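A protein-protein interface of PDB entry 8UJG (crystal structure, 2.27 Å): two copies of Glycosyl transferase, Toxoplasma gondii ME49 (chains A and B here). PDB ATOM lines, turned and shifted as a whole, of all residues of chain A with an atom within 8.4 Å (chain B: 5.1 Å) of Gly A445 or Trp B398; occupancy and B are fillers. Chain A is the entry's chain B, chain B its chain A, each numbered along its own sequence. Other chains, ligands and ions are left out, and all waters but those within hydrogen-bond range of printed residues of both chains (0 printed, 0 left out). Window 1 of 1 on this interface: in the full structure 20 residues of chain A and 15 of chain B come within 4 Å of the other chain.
The side-chain carboxylate (OD1) of Asp B303 lies within hydrogen-bond range of the backbone NH (N) of Asp A462, at 2.7 Å. The side-chain carboxylate (OD1) of Asp B303 is in hydrogen-bond range of the backbone NH (N) of Thr A463 (3.3 Å).
The side-chain amino group (NZ) of Lys B402 sits at hydrogen-bond distance from the backbone carbonyl oxygen (O) of Asp B303, at 3.2 Å. O of Gly B305 lies within hydrogen-bond range of NH2 of Arg B395 (2.8 Å). The side-chain amide oxygen (OD1) of Asn A443 is in hydrogen-bond range of the backbone NH (N) of Gly A445 (2.7 Å). The backbone carbonyl oxygen of Ser A448 lies within hydrogen-bond range of a ring nitrogen (ND1) of His A451 (3.2 Å). The backbone NH (N) of Leu A491 is in hydrogen-bond range of the backbone carbonyl oxygen (O) of His A451, 2.7 Å away. The side-chain sulfur of Cys B404 is disulfide-bonded to the side-chain sulfur of Cys B328, at 2.0 Å.
Among the printed residues, merely in contact across the chains: Gly A445 with Trp B398, Trp A446 with Lys B394, Trp A446 with Arg B395, Ser A448 with Arg B401, His A451 with Lys B394 and Asn A479 with Arg B401.
Of the printed residues of chain A, Arg B395 touches Trp A446 (3.1 Å). Of the printed residues of chain B, Asp A462 touches Asp B303. Of the printed residues of chain A, Asp B303 touches Asp A462 and Thr A463. Printed residues of chain B within 4 Å of Asn A479: Arg B401 (3.4 Å). The nearest residue of chain A that does not touch Trp B398 is Trp A446 (4.03 Å).
Hydrophobic or aromatic side chains of chain A that line the printed part of chain B: Trp A446 and His A451. Among the printed residues, no Asp or Glu carboxylate lies within 4 Å of a Lys or Arg side-chain nitrogen of the other chain.
No position is printed for both chains. Of the 8 pairs that touch across the chains among the printed residues, none has its exchanged pair printed and touching as well.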
ATOM      1  N   ASP A 442      16.360  -0.681 -18.374  1.00  0.00           N
ATOM      2  CA  ASP A 442      15.165  -0.070 -17.807  1.00  0.00           C
ATOM      3  C   ASP A 442      13.979  -0.971 -18.101  1.00  0.00           C
ATOM      4  O   ASP A 442      13.691  -1.255 -19.268  1.00  0.00           O
ATOM      5  CB  ASP A 442      14.942   1.328 -18.394  1.00  0.00           C
ATOM      6  CG  ASP A 442      13.997   2.169 -17.560  1.00  0.00           C
ATOM      7  OD1 ASP A 442      13.057   1.602 -16.964  1.00  0.00           O
ATOM      8  OD2 ASP A 442      14.199   3.401 -17.504  1.00  0.00           O
ATOM      9  N   ASN A 443      13.287  -1.417 -17.051  1.00  0.00           N
ATOM     10  CA  ASN A 443      12.090  -2.226 -17.257  1.00  0.00           C
ATOM     11  C   ASN A 443      10.949  -1.425 -17.868  1.00  0.00           C
ATOM     12  O   ASN A 443       9.894  -2.000 -18.149  1.00  0.00           O
ATOM     13  CB  ASN A 443      11.636  -2.866 -15.938  1.00  0.00           C
ATOM     14  CG  ASN A 443      11.160  -1.848 -14.908  1.00  0.00           C
ATOM     15  OD1 ASN A 443      10.727  -0.745 -15.246  1.00  0.00           O
ATOM     16  ND2 ASN A 443      11.229  -2.229 -13.636  1.00  0.00           N
ATOM     17  N   MET A 444      11.139  -0.120 -18.065  1.00  0.00           N
ATOM     18  CA  MET A 444      10.171   0.733 -18.751  1.00  0.00           C
ATOM     19  C   MET A 444       8.864   0.845 -17.977  1.00  0.00           C
ATOM     20  O   MET A 444       7.792   1.003 -18.565  1.00  0.00           O
ATOM     21  CB  MET A 444       9.906   0.237 -20.175  1.00  0.00           C
ATOM     22  CG  MET A 444      11.140   0.177 -21.059  1.00  0.00           C
ATOM     23  SD  MET A 444      12.093   1.700 -20.916  1.00  0.00           S
ATOM     24  CE  MET A 444      10.911   2.877 -21.561  1.00  0.00           C
ATOM     25  N   GLY A 445       8.957   0.785 -16.650  1.00  0.00           N
ATOM     26  CA  GLY A 445       7.825   0.942 -15.765  1.00  0.00           C
ATOM     27  C   GLY A 445       6.922  -0.263 -15.659  1.00  0.00           C
ATOM     28  O   GLY A 445       5.885  -0.182 -14.989  1.00  0.00           O
ATOM     29  N   TRP A 446       7.270  -1.371 -16.307  1.00  0.00           N
ATOM     30  CA  TRP A 446       6.502  -2.612 -16.259  1.00  0.00           C
ATOM     31  C   TRP A 446       7.375  -3.748 -15.746  1.00  0.00           C
ATOM     32  O   TRP A 446       8.009  -4.460 -16.526  1.00  0.00           O
ATOM     33  CB  TRP A 446       5.912  -2.904 -17.630  1.00  0.00           C
ATOM     34  CG  TRP A 446       4.877  -1.902 -17.954  1.00  0.00           C
ATOM     35  CD1 TRP A 446       4.953  -0.889 -18.863  1.00  0.00           C
ATOM     36  CD2 TRP A 446       3.587  -1.815 -17.359  1.00  0.00           C
ATOM     37  NE1 TRP A 446       3.783  -0.168 -18.862  1.00  0.00           N
ATOM     38  CE2 TRP A 446       2.926  -0.722 -17.948  1.00  0.00           C
ATOM     39  CE3 TRP A 446       2.924  -2.559 -16.382  1.00  0.00           C
ATOM     40  CZ2 TRP A 446       1.637  -0.357 -17.593  1.00  0.00           C
ATOM     41  CZ3 TRP A 446       1.659  -2.197 -16.032  1.00  0.00           C
ATOM     42  CH2 TRP A 446       1.022  -1.105 -16.634  1.00  0.00           C
ATOM     43  N   ALA A 447       7.419  -3.908 -14.421  1.00  0.00           N
ATOM     44  CA  ALA A 447       8.109  -5.050 -13.835  1.00  0.00           C
ATOM     45  C   ALA A 447       7.302  -6.327 -14.013  1.00  0.00           C
ATOM     46  O   ALA A 447       7.790  -7.407 -13.657  1.00  0.00           O
ATOM     47  CB  ALA A 447       8.405  -4.807 -12.356  1.00  0.00           C
ATOM     48  N   SER A 448       6.084  -6.224 -14.541  1.00  0.00           N
ATOM     49  CA  SER A 448       5.301  -7.402 -14.860  1.00  0.00           C
ATOM     50  C   SER A 448       5.884  -8.103 -16.083  1.00  0.00           C
ATOM     51  O   SER A 448       6.451  -7.460 -16.969  1.00  0.00           O
ATOM     52  CB  SER A 448       3.854  -7.026 -15.154  1.00  0.00           C
ATOM     53  OG  SER A 448       3.098  -8.170 -15.510  1.00  0.00           O
ATOM     54  N   HIS A 451       6.685  -7.572 -21.317  1.00  0.00           N
ATOM     55  CA  HIS A 451       6.996  -6.331 -22.009  1.00  0.00           C
ATOM     56  C   HIS A 451       8.482  -6.247 -22.331  1.00  0.00           C
ATOM     57  O   HIS A 451       9.309  -6.971 -21.771  1.00  0.00           O
ATOM     58  CB  HIS A 451       6.590  -5.115 -21.173  1.00  0.00           C
ATOM     59  CG  HIS A 451       5.239  -5.241 -20.549  1.00  0.00           C
ATOM     60  ND1 HIS A 451       5.039  -5.848 -19.328  1.00  0.00           N
ATOM     61  CD2 HIS A 451       4.015  -4.866 -20.988  1.00  0.00           C
ATOM     62  CE1 HIS A 451       3.751  -5.824 -19.033  1.00  0.00           C
ATOM     63  NE2 HIS A 451       3.109  -5.236 -20.025  1.00  0.00           N
ATOM     64  N   ALA A 452       8.808  -5.332 -23.240  1.00  0.00           N
ATOM     65  CA  ALA A 452      10.181  -5.144 -23.678  1.00  0.00           C
ATOM     66  C   ALA A 452      10.970  -4.329 -22.662  1.00  0.00           C
ATOM     67  O   ALA A 452      10.440  -3.433 -21.999  1.00  0.00           O
ATOM     68  CB  ALA A 452      10.216  -4.446 -25.038  1.00  0.00           C
ATOM     69  N   VAL A 453      12.249  -4.653 -22.544  1.00  0.00           N
ATOM     70  CA  VAL A 453      13.179  -3.906 -21.707  1.00  0.00           C
ATOM     71  C   VAL A 453      13.822  -2.822 -22.559  1.00  0.00           C
ATOM     72  O   VAL A 453      14.111  -3.033 -23.742  1.00  0.00           O
ATOM     73  CB  VAL A 453      14.238  -4.841 -21.096  1.00  0.00           C
ATOM     74  CG1 VAL A 453      15.290  -4.042 -20.344  1.00  0.00           C
ATOM     75  CG2 VAL A 453      13.577  -5.861 -20.183  1.00  0.00           C
ATOM     76  N   GLY A 454      14.046  -1.652 -21.959  1.00  0.00           N
ATOM     77  CA  GLY A 454      14.567  -0.506 -22.664  1.00  0.00           C
ATOM     78  C   GLY A 454      15.950  -0.083 -22.189  1.00  0.00           C
ATOM     79  O   GLY A 454      16.480  -0.561 -21.188  1.00  0.00           O
ATOM     80  N   GLU A 456      17.827   3.478 -21.234  1.00  0.00           N
ATOM     81  CA  GLU A 456      17.525   4.855 -20.875  1.00  0.00           C
ATOM     82  C   GLU A 456      18.677   5.415 -20.055  1.00  0.00           C
ATOM     83  O   GLU A 456      19.531   4.675 -19.561  1.00  0.00           O
ATOM     84  CB  GLU A 456      16.213   4.952 -20.085  1.00  0.00           C
ATOM     85  CG  GLU A 456      15.003   4.376 -20.804  1.00  0.00           C
ATOM     86  CD  GLU A 456      14.612   5.181 -22.027  1.00  0.00           C
ATOM     87  OE1 GLU A 456      15.043   6.348 -22.136  1.00  0.00           O
ATOM     88  OE2 GLU A 456      13.874   4.646 -22.880  1.00  0.00           O
ATOM     89  N   HIS A 459      19.265   6.945 -13.749  1.00  0.00           N
ATOM     90  CA  HIS A 459      18.794   7.874 -12.731  1.00  0.00           C
ATOM     91  C   HIS A 459      18.780   7.275 -11.328  1.00  0.00           C
ATOM     92  O   HIS A 459      18.482   7.998 -10.371  1.00  0.00           O
ATOM     93  CB  HIS A 459      17.386   8.389 -13.077  1.00  0.00           C
ATOM     94  CG  HIS A 459      16.402   7.308 -13.400  1.00  0.00           C
ATOM     95  ND1 HIS A 459      16.143   6.258 -12.547  1.00  0.00           N
ATOM     96  CD2 HIS A 459      15.596   7.126 -14.474  1.00  0.00           C
ATOM     97  CE1 HIS A 459      15.231   5.468 -13.086  1.00  0.00           C
ATOM     98  NE2 HIS A 459      14.882   5.974 -14.256  1.00  0.00           N
ATOM     99  N   ASP A 462      14.364   2.544  -8.732  1.00  0.00           N
ATOM    100  CA  ASP A 462      14.101   1.110  -8.682  1.00  0.00           C
ATOM    101  C   ASP A 462      13.821   0.535 -10.065  1.00  0.00           C
ATOM    102  O   ASP A 462      14.098  -0.646 -10.313  1.00  0.00           O
ATOM    103  CB  ASP A 462      12.926   0.823  -7.742  1.00  0.00           C
ATOM    104  CG  ASP A 462      13.367   0.619  -6.307  1.00  0.00           C
ATOM    105  OD1 ASP A 462      14.481   1.065  -5.959  1.00  0.00           O
ATOM    106  OD2 ASP A 462      12.607   0.001  -5.531  1.00  0.00           O
ATOM    107  N   THR A 463      13.290   1.347 -10.980  1.00  0.00           N
ATOM    108  CA  THR A 463      12.961   0.862 -12.314  1.00  0.00           C
ATOM    109  C   THR A 463      14.190   0.434 -13.105  1.00  0.00           C
ATOM    110  O   THR A 463      14.041  -0.221 -14.144  1.00  0.00           O
ATOM    111  CB  THR A 463      12.214   1.942 -13.102  1.00  0.00           C
ATOM    112  OG1 THR A 463      13.077   3.067 -13.316  1.00  0.00           O
ATOM    113  CG2 THR A 463      10.977   2.399 -12.341  1.00  0.00           C
ATOM    114  N   GLN A 464      15.393   0.783 -12.645  1.00  0.00           N
ATOM    115  CA  GLN A 464      16.619   0.498 -13.378  1.00  0.00           C
ATOM    116  C   GLN A 464      17.581  -0.395 -12.604  1.00  0.00           C
ATOM    117  O   GLN A 464      18.738  -0.536 -13.013  1.00  0.00           O
ATOM    118  CB  GLN A 464      17.321   1.806 -13.760  1.00  0.00           C
ATOM    119  CG  GLN A 464      16.656   2.551 -14.907  1.00  0.00           C
ATOM    120  CD  GLN A 464      17.298   3.900 -15.170  1.00  0.00           C
ATOM    121  OE1 GLN A 464      18.172   4.339 -14.423  1.00  0.00           O
ATOM    122  NE2 GLN A 464      16.873   4.559 -16.242  1.00  0.00           N
ATOM    123  N   ASN A 479      11.968  -5.342  -8.252  1.00  0.00           N
ATOM    124  CA  ASN A 479      10.597  -5.256  -7.763  1.00  0.00           C
ATOM    125  C   ASN A 479       9.724  -6.431  -8.192  1.00  0.00           C
ATOM    126  O   ASN A 479       8.516  -6.403  -7.930  1.00  0.00           O
ATOM    127  CB  ASN A 479       9.954  -3.947  -8.230  1.00  0.00           C
ATOM    128  CG  ASN A 479      10.726  -2.724  -7.772  1.00  0.00           C
ATOM    129  OD1 ASN A 479      11.015  -1.828  -8.564  1.00  0.00           O
ATOM    130  ND2 ASN A 479      11.068  -2.683  -6.488  1.00  0.00           N
ATOM    131  N   LEU A 491      10.907  -8.997 -21.034  1.00  0.00           N
ATOM    132  CA  LEU A 491      10.634  -9.725 -19.800  1.00  0.00           C
ATOM    133  C   LEU A 491       9.518 -10.749 -19.964  1.00  0.00           C
ATOM    134  O   LEU A 491       8.582 -10.564 -20.747  1.00  0.00           O
ATOM    135  CB  LEU A 491      10.261  -8.750 -18.676  1.00  0.00           C
ATOM    136  CG  LEU A 491      11.338  -7.779 -18.189  1.00  0.00           C
ATOM    137  CD1 LEU A 491      10.824  -6.942 -17.032  1.00  0.00           C
ATOM    138  CD2 LEU A 491      12.579  -8.545 -17.759  1.00  0.00           C
ATOM    139  N   ASP B 303       9.712   5.803 -10.222  1.00  0.00           N
ATOM    140  CA  ASP B 303       9.333   4.783  -9.252  1.00  0.00           C
ATOM    141  C   ASP B 303       7.850   4.860  -8.902  1.00  0.00           C
ATOM    142  O   ASP B 303       7.255   3.849  -8.514  1.00  0.00           O
ATOM    143  CB  ASP B 303      10.172   4.921  -7.978  1.00  0.00           C
ATOM    144  CG  ASP B 303      11.624   4.511  -8.179  1.00  0.00           C
ATOM    145  OD1 ASP B 303      11.904   3.713  -9.099  1.00  0.00           O
ATOM    146  OD2 ASP B 303      12.487   4.980  -7.402  1.00  0.00           O
ATOM    147  N   VAL B 304       7.243   6.041  -9.030  1.00  0.00           N
ATOM    148  CA  VAL B 304       5.843   6.239  -8.676  1.00  0.00           C
ATOM    149  C   VAL B 304       4.928   6.151  -9.894  1.00  0.00           C
ATOM    150  O   VAL B 304       3.765   6.559  -9.823  1.00  0.00           O
ATOM    151  CB  VAL B 304       5.652   7.576  -7.937  1.00  0.00           C
ATOM    152  CG1 VAL B 304       5.522   8.731  -8.923  1.00  0.00           C
ATOM    153  CG2 VAL B 304       4.446   7.507  -7.009  1.00  0.00           C
ATOM    154  N   GLY B 305       5.425   5.623 -11.013  1.00  0.00           N
ATOM    155  CA  GLY B 305       4.610   5.379 -12.184  1.00  0.00           C
ATOM    156  C   GLY B 305       4.704   6.431 -13.266  1.00  0.00           C
ATOM    157  O   GLY B 305       4.021   6.297 -14.289  1.00  0.00           O
ATOM    158  N   ARG B 324      -2.492   9.046  -8.136  1.00  0.00           N
ATOM    159  CA  ARG B 324      -1.470   8.009  -8.044  1.00  0.00           C
ATOM    160  C   ARG B 324      -0.336   8.439  -7.124  1.00  0.00           C
ATOM    161  O   ARG B 324       0.176   7.633  -6.338  1.00  0.00           O
ATOM    162  CB  ARG B 324      -0.940   7.681  -9.440  1.00  0.00           C
ATOM    163  CG  ARG B 324       0.291   6.787  -9.453  1.00  0.00           C
ATOM    164  CD  ARG B 324       0.595   6.286 -10.855  1.00  0.00           C
ATOM    165  NE  ARG B 324       0.442   7.323 -11.868  1.00  0.00           N
ATOM    166  CZ  ARG B 324       1.386   8.194 -12.201  1.00  0.00           C
ATOM    167  NH1 ARG B 324       2.570   8.191 -11.608  1.00  0.00           N
ATOM    168  NH2 ARG B 324       1.140   9.087 -13.155  1.00  0.00           N
ATOM    169  N   CYS B 328       0.478   6.204  -3.751  1.00  0.00           N
ATOM    170  CA  CYS B 328       1.624   5.319  -3.905  1.00  0.00           C
ATOM    171  C   CYS B 328       2.884   5.870  -3.241  1.00  0.00           C
ATOM    172  O   CYS B 328       4.000   5.592  -3.691  1.00  0.00           O
ATOM    173  CB  CYS B 328       1.874   5.043  -5.388  1.00  0.00           C
ATOM    174  SG  CYS B 328       0.394   4.532  -6.310  1.00  0.00           S
ATOM    175  N   TRP B 368      -8.003   4.861 -10.508  1.00  0.00           N
ATOM    176  CA  TRP B 368      -7.478   5.223  -9.201  1.00  0.00           C
ATOM    177  C   TRP B 368      -8.549   5.729  -8.251  1.00  0.00           C
ATOM    178  O   TRP B 368      -8.223   6.133  -7.131  1.00  0.00           O
ATOM    179  CB  TRP B 368      -6.385   6.280  -9.378  1.00  0.00           C
ATOM    180  CG  TRP B 368      -5.332   5.796 -10.308  1.00  0.00           C
ATOM    181  CD1 TRP B 368      -5.334   5.887 -11.669  1.00  0.00           C
ATOM    182  CD2 TRP B 368      -4.138   5.099  -9.953  1.00  0.00           C
ATOM    183  NE1 TRP B 368      -4.205   5.302 -12.183  1.00  0.00           N
ATOM    184  CE2 TRP B 368      -3.453   4.811 -11.148  1.00  0.00           C
ATOM    185  CE3 TRP B 368      -3.575   4.696  -8.739  1.00  0.00           C
ATOM    186  CZ2 TRP B 368      -2.238   4.138 -11.165  1.00  0.00           C
ATOM    187  CZ3 TRP B 368      -2.365   4.034  -8.759  1.00  0.00           C
ATOM    188  CH2 TRP B 368      -1.710   3.759  -9.963  1.00  0.00           C
ATOM    189  N   LYS B 394      -3.058  -3.631 -17.079  1.00  0.00           N
ATOM    190  CA  LYS B 394      -1.668  -3.712 -16.655  1.00  0.00           C
ATOM    191  C   LYS B 394      -1.362  -2.612 -15.650  1.00  0.00           C
ATOM    192  O   LYS B 394      -0.666  -2.847 -14.656  1.00  0.00           O
ATOM    193  CB  LYS B 394      -0.757  -3.642 -17.876  1.00  0.00           C
ATOM    194  CG  LYS B 394      -1.019  -4.776 -18.861  1.00  0.00           C
ATOM    195  CD  LYS B 394       0.048  -4.903 -19.928  1.00  0.00           C
ATOM    196  CE  LYS B 394      -0.448  -5.745 -21.094  1.00  0.00           C
ATOM    197  NZ  LYS B 394      -0.762  -7.130 -20.637  1.00  0.00           N
ATOM    198  N   ARG B 395      -1.932  -1.421 -15.854  1.00  0.00           N
ATOM    199  CA  ARG B 395      -1.749  -0.341 -14.889  1.00  0.00           C
ATOM    200  C   ARG B 395      -2.333  -0.720 -13.536  1.00  0.00           C
ATOM    201  O   ARG B 395      -1.794  -0.332 -12.494  1.00  0.00           O
ATOM    202  CB  ARG B 395      -2.397   0.942 -15.413  1.00  0.00           C
ATOM    203  CG  ARG B 395      -1.874   2.228 -14.789  1.00  0.00           C
ATOM    204  CD  ARG B 395      -0.533   2.643 -15.380  1.00  0.00           C
ATOM    205  NE  ARG B 395      -0.159   3.988 -14.954  1.00  0.00           N
ATOM    206  CZ  ARG B 395       1.086   4.432 -14.850  1.00  0.00           C
ATOM    207  NH1 ARG B 395       2.123   3.659 -15.127  1.00  0.00           N
ATOM    208  NH2 ARG B 395       1.295   5.685 -14.458  1.00  0.00           N
ATOM    209  N   ARG B 396      -3.421  -1.493 -13.537  1.00  0.00           N
ATOM    210  CA  ARG B 396      -4.008  -1.959 -12.287  1.00  0.00           C
ATOM    211  C   ARG B 396      -3.063  -2.909 -11.559  1.00  0.00           C
ATOM    212  O   ARG B 396      -2.900  -2.819 -10.337  1.00  0.00           O
ATOM    213  CB  ARG B 396      -5.336  -2.657 -12.575  1.00  0.00           C
ATOM    214  CG  ARG B 396      -6.277  -2.744 -11.388  1.00  0.00           C
ATOM    215  CD  ARG B 396      -7.412  -3.719 -11.664  1.00  0.00           C
ATOM    216  NE  ARG B 396      -8.378  -3.210 -12.632  1.00  0.00           N
ATOM    217  CZ  ARG B 396      -9.444  -2.480 -12.330  1.00  0.00           C
ATOM    218  NH1 ARG B 396      -9.709  -2.119 -11.086  1.00  0.00           N
ATOM    219  NH2 ARG B 396     -10.268  -2.104 -13.305  1.00  0.00           N
ATOM    220  N   GLU B 397      -2.428  -3.826 -12.296  1.00  0.00           N
ATOM    221  CA  GLU B 397      -1.472  -4.738 -11.677  1.00  0.00           C
ATOM    222  C   GLU B 397      -0.306  -3.971 -11.066  1.00  0.00           C
ATOM    223  O   GLU B 397       0.166  -4.308  -9.973  1.00  0.00           O
ATOM    224  CB  GLU B 397      -0.968  -5.753 -12.703  1.00  0.00           C
ATOM    225  CG  GLU B 397      -0.905  -7.179 -12.175  1.00  0.00           C
ATOM    226  CD  GLU B 397      -2.274  -7.823 -12.070  1.00  0.00           C
ATOM    227  OE1 GLU B 397      -2.918  -8.025 -13.121  1.00  0.00           O
ATOM    228  OE2 GLU B 397      -2.710  -8.118 -10.938  1.00  0.00           O
ATOM    229  N   TRP B 398       0.180  -2.944 -11.765  1.00  0.00           N
ATOM    230  CA  TRP B 398       1.232  -2.103 -11.207  1.00  0.00           C
ATOM    231  C   TRP B 398       0.799  -1.512  -9.871  1.00  0.00           C
ATOM    232  O   TRP B 398       1.570  -1.503  -8.905  1.00  0.00           O
ATOM    233  CB  TRP B 398       1.581  -0.987 -12.191  1.00  0.00           C
ATOM    234  CG  TRP B 398       2.709  -0.112 -11.739  1.00  0.00           C
ATOM    235  CD1 TRP B 398       4.022  -0.227 -12.084  1.00  0.00           C
ATOM    236  CD2 TRP B 398       2.627   1.006 -10.846  1.00  0.00           C
ATOM    237  NE1 TRP B 398       4.762   0.752 -11.469  1.00  0.00           N
ATOM    238  CE2 TRP B 398       3.930   1.522 -10.701  1.00  0.00           C
ATOM    239  CE3 TRP B 398       1.578   1.622 -10.157  1.00  0.00           C
ATOM    240  CZ2 TRP B 398       4.212   2.623  -9.898  1.00  0.00           C
ATOM    241  CZ3 TRP B 398       1.860   2.716  -9.359  1.00  0.00           C
ATOM    242  CH2 TRP B 398       3.166   3.206  -9.235  1.00  0.00           C
ATOM    243  N   ARG B 399      -0.437  -1.010  -9.801  1.00  0.00           N
ATOM    244  CA  ARG B 399      -0.939  -0.432  -8.560  1.00  0.00           C
ATOM    245  C   ARG B 399      -0.922  -1.448  -7.426  1.00  0.00           C
ATOM    246  O   ARG B 399      -0.612  -1.104  -6.279  1.00  0.00           O
ATOM    247  CB  ARG B 399      -2.352   0.106  -8.782  1.00  0.00           C
ATOM    248  CG  ARG B 399      -2.930   0.869  -7.606  1.00  0.00           C
ATOM    249  CD  ARG B 399      -4.343   1.334  -7.916  1.00  0.00           C
ATOM    250  NE  ARG B 399      -4.966   2.018  -6.788  1.00  0.00           N
ATOM    251  CZ  ARG B 399      -6.276   2.135  -6.612  1.00  0.00           C
ATOM    252  NH1 ARG B 399      -7.139   1.602  -7.462  1.00  0.00           N
ATOM    253  NH2 ARG B 399      -6.731   2.798  -5.553  1.00  0.00           N
ATOM    254  N   LYS B 400      -1.252  -2.707  -7.724  1.00  0.00           N
ATOM    255  CA  LYS B 400      -1.250  -3.734  -6.687  1.00  0.00           C
ATOM    256  C   LYS B 400       0.169  -4.050  -6.230  1.00  0.00           C
ATOM    257  O   LYS B 400       0.455  -4.061  -5.027  1.00  0.00           O
ATOM    258  CB  LYS B 400      -1.949  -4.997  -7.195  1.00  0.00           C
ATOM    259  N   ARG B 401       1.076  -4.309  -7.179  1.00  0.00           N
ATOM    260  CA  ARG B 401       2.449  -4.647  -6.814  1.00  0.00           C
ATOM    261  C   ARG B 401       3.068  -3.533  -5.979  1.00  0.00           C
ATOM    262  O   ARG B 401       3.728  -3.791  -4.966  1.00  0.00           O
ATOM    263  CB  ARG B 401       3.288  -4.878  -8.072  1.00  0.00           C
ATOM    264  CG  ARG B 401       4.755  -5.214  -7.794  1.00  0.00           C
ATOM    265  CD  ARG B 401       5.576  -5.254  -9.077  1.00  0.00           C
ATOM    266  NE  ARG B 401       4.940  -6.085 -10.089  1.00  0.00           N
ATOM    267  CZ  ARG B 401       4.242  -5.608 -11.114  1.00  0.00           C
ATOM    268  NH1 ARG B 401       4.083  -4.308 -11.299  1.00  0.00           N
ATOM    269  NH2 ARG B 401       3.665  -6.459 -11.953  1.00  0.00           N
ATOM    270  N   LYS B 402       2.871  -2.284  -6.403  1.00  0.00           N
ATOM    271  CA  LYS B 402       3.405  -1.142  -5.674  1.00  0.00           C
ATOM    272  C   LYS B 402       2.793  -1.010  -4.287  1.00  0.00           C
ATOM    273  O   LYS B 402       3.400  -0.383  -3.412  1.00  0.00           O
ATOM    274  CB  LYS B 402       3.161   0.134  -6.490  1.00  0.00           C
ATOM    275  CG  LYS B 402       3.612   1.433  -5.832  1.00  0.00           C
ATOM    276  CD  LYS B 402       5.120   1.607  -5.882  1.00  0.00           C
ATOM    277  CE  LYS B 402       5.542   2.860  -5.131  1.00  0.00           C
ATOM    278  NZ  LYS B 402       6.965   3.217  -5.368  1.00  0.00           N
ATOM    279  N   GLY B 403       1.619  -1.592  -4.061  1.00  0.00           N
ATOM    280  CA  GLY B 403       0.966  -1.473  -2.774  1.00  0.00           C
ATOM    281  C   GLY B 403       0.303  -0.138  -2.532  1.00  0.00           C
ATOM    282  O   GLY B 403       0.253   0.323  -1.387  1.00  0.00           O
ATOM    283  N   CYS B 404      -0.206   0.504  -3.581  1.00  0.00           N
ATOM    284  CA  CYS B 404      -0.815   1.818  -3.429  1.00  0.00           C
ATOM    285  C   CYS B 404      -2.054   1.735  -2.545  1.00  0.00           C
ATOM    286  O   CYS B 404      -2.748   0.717  -2.499  1.00  0.00           O
ATOM    287  CB  CYS B 404      -1.185   2.395  -4.795  1.00  0.00           C
ATOM    288  SG  CYS B 404       0.199   2.537  -5.958  1.00  0.00           S
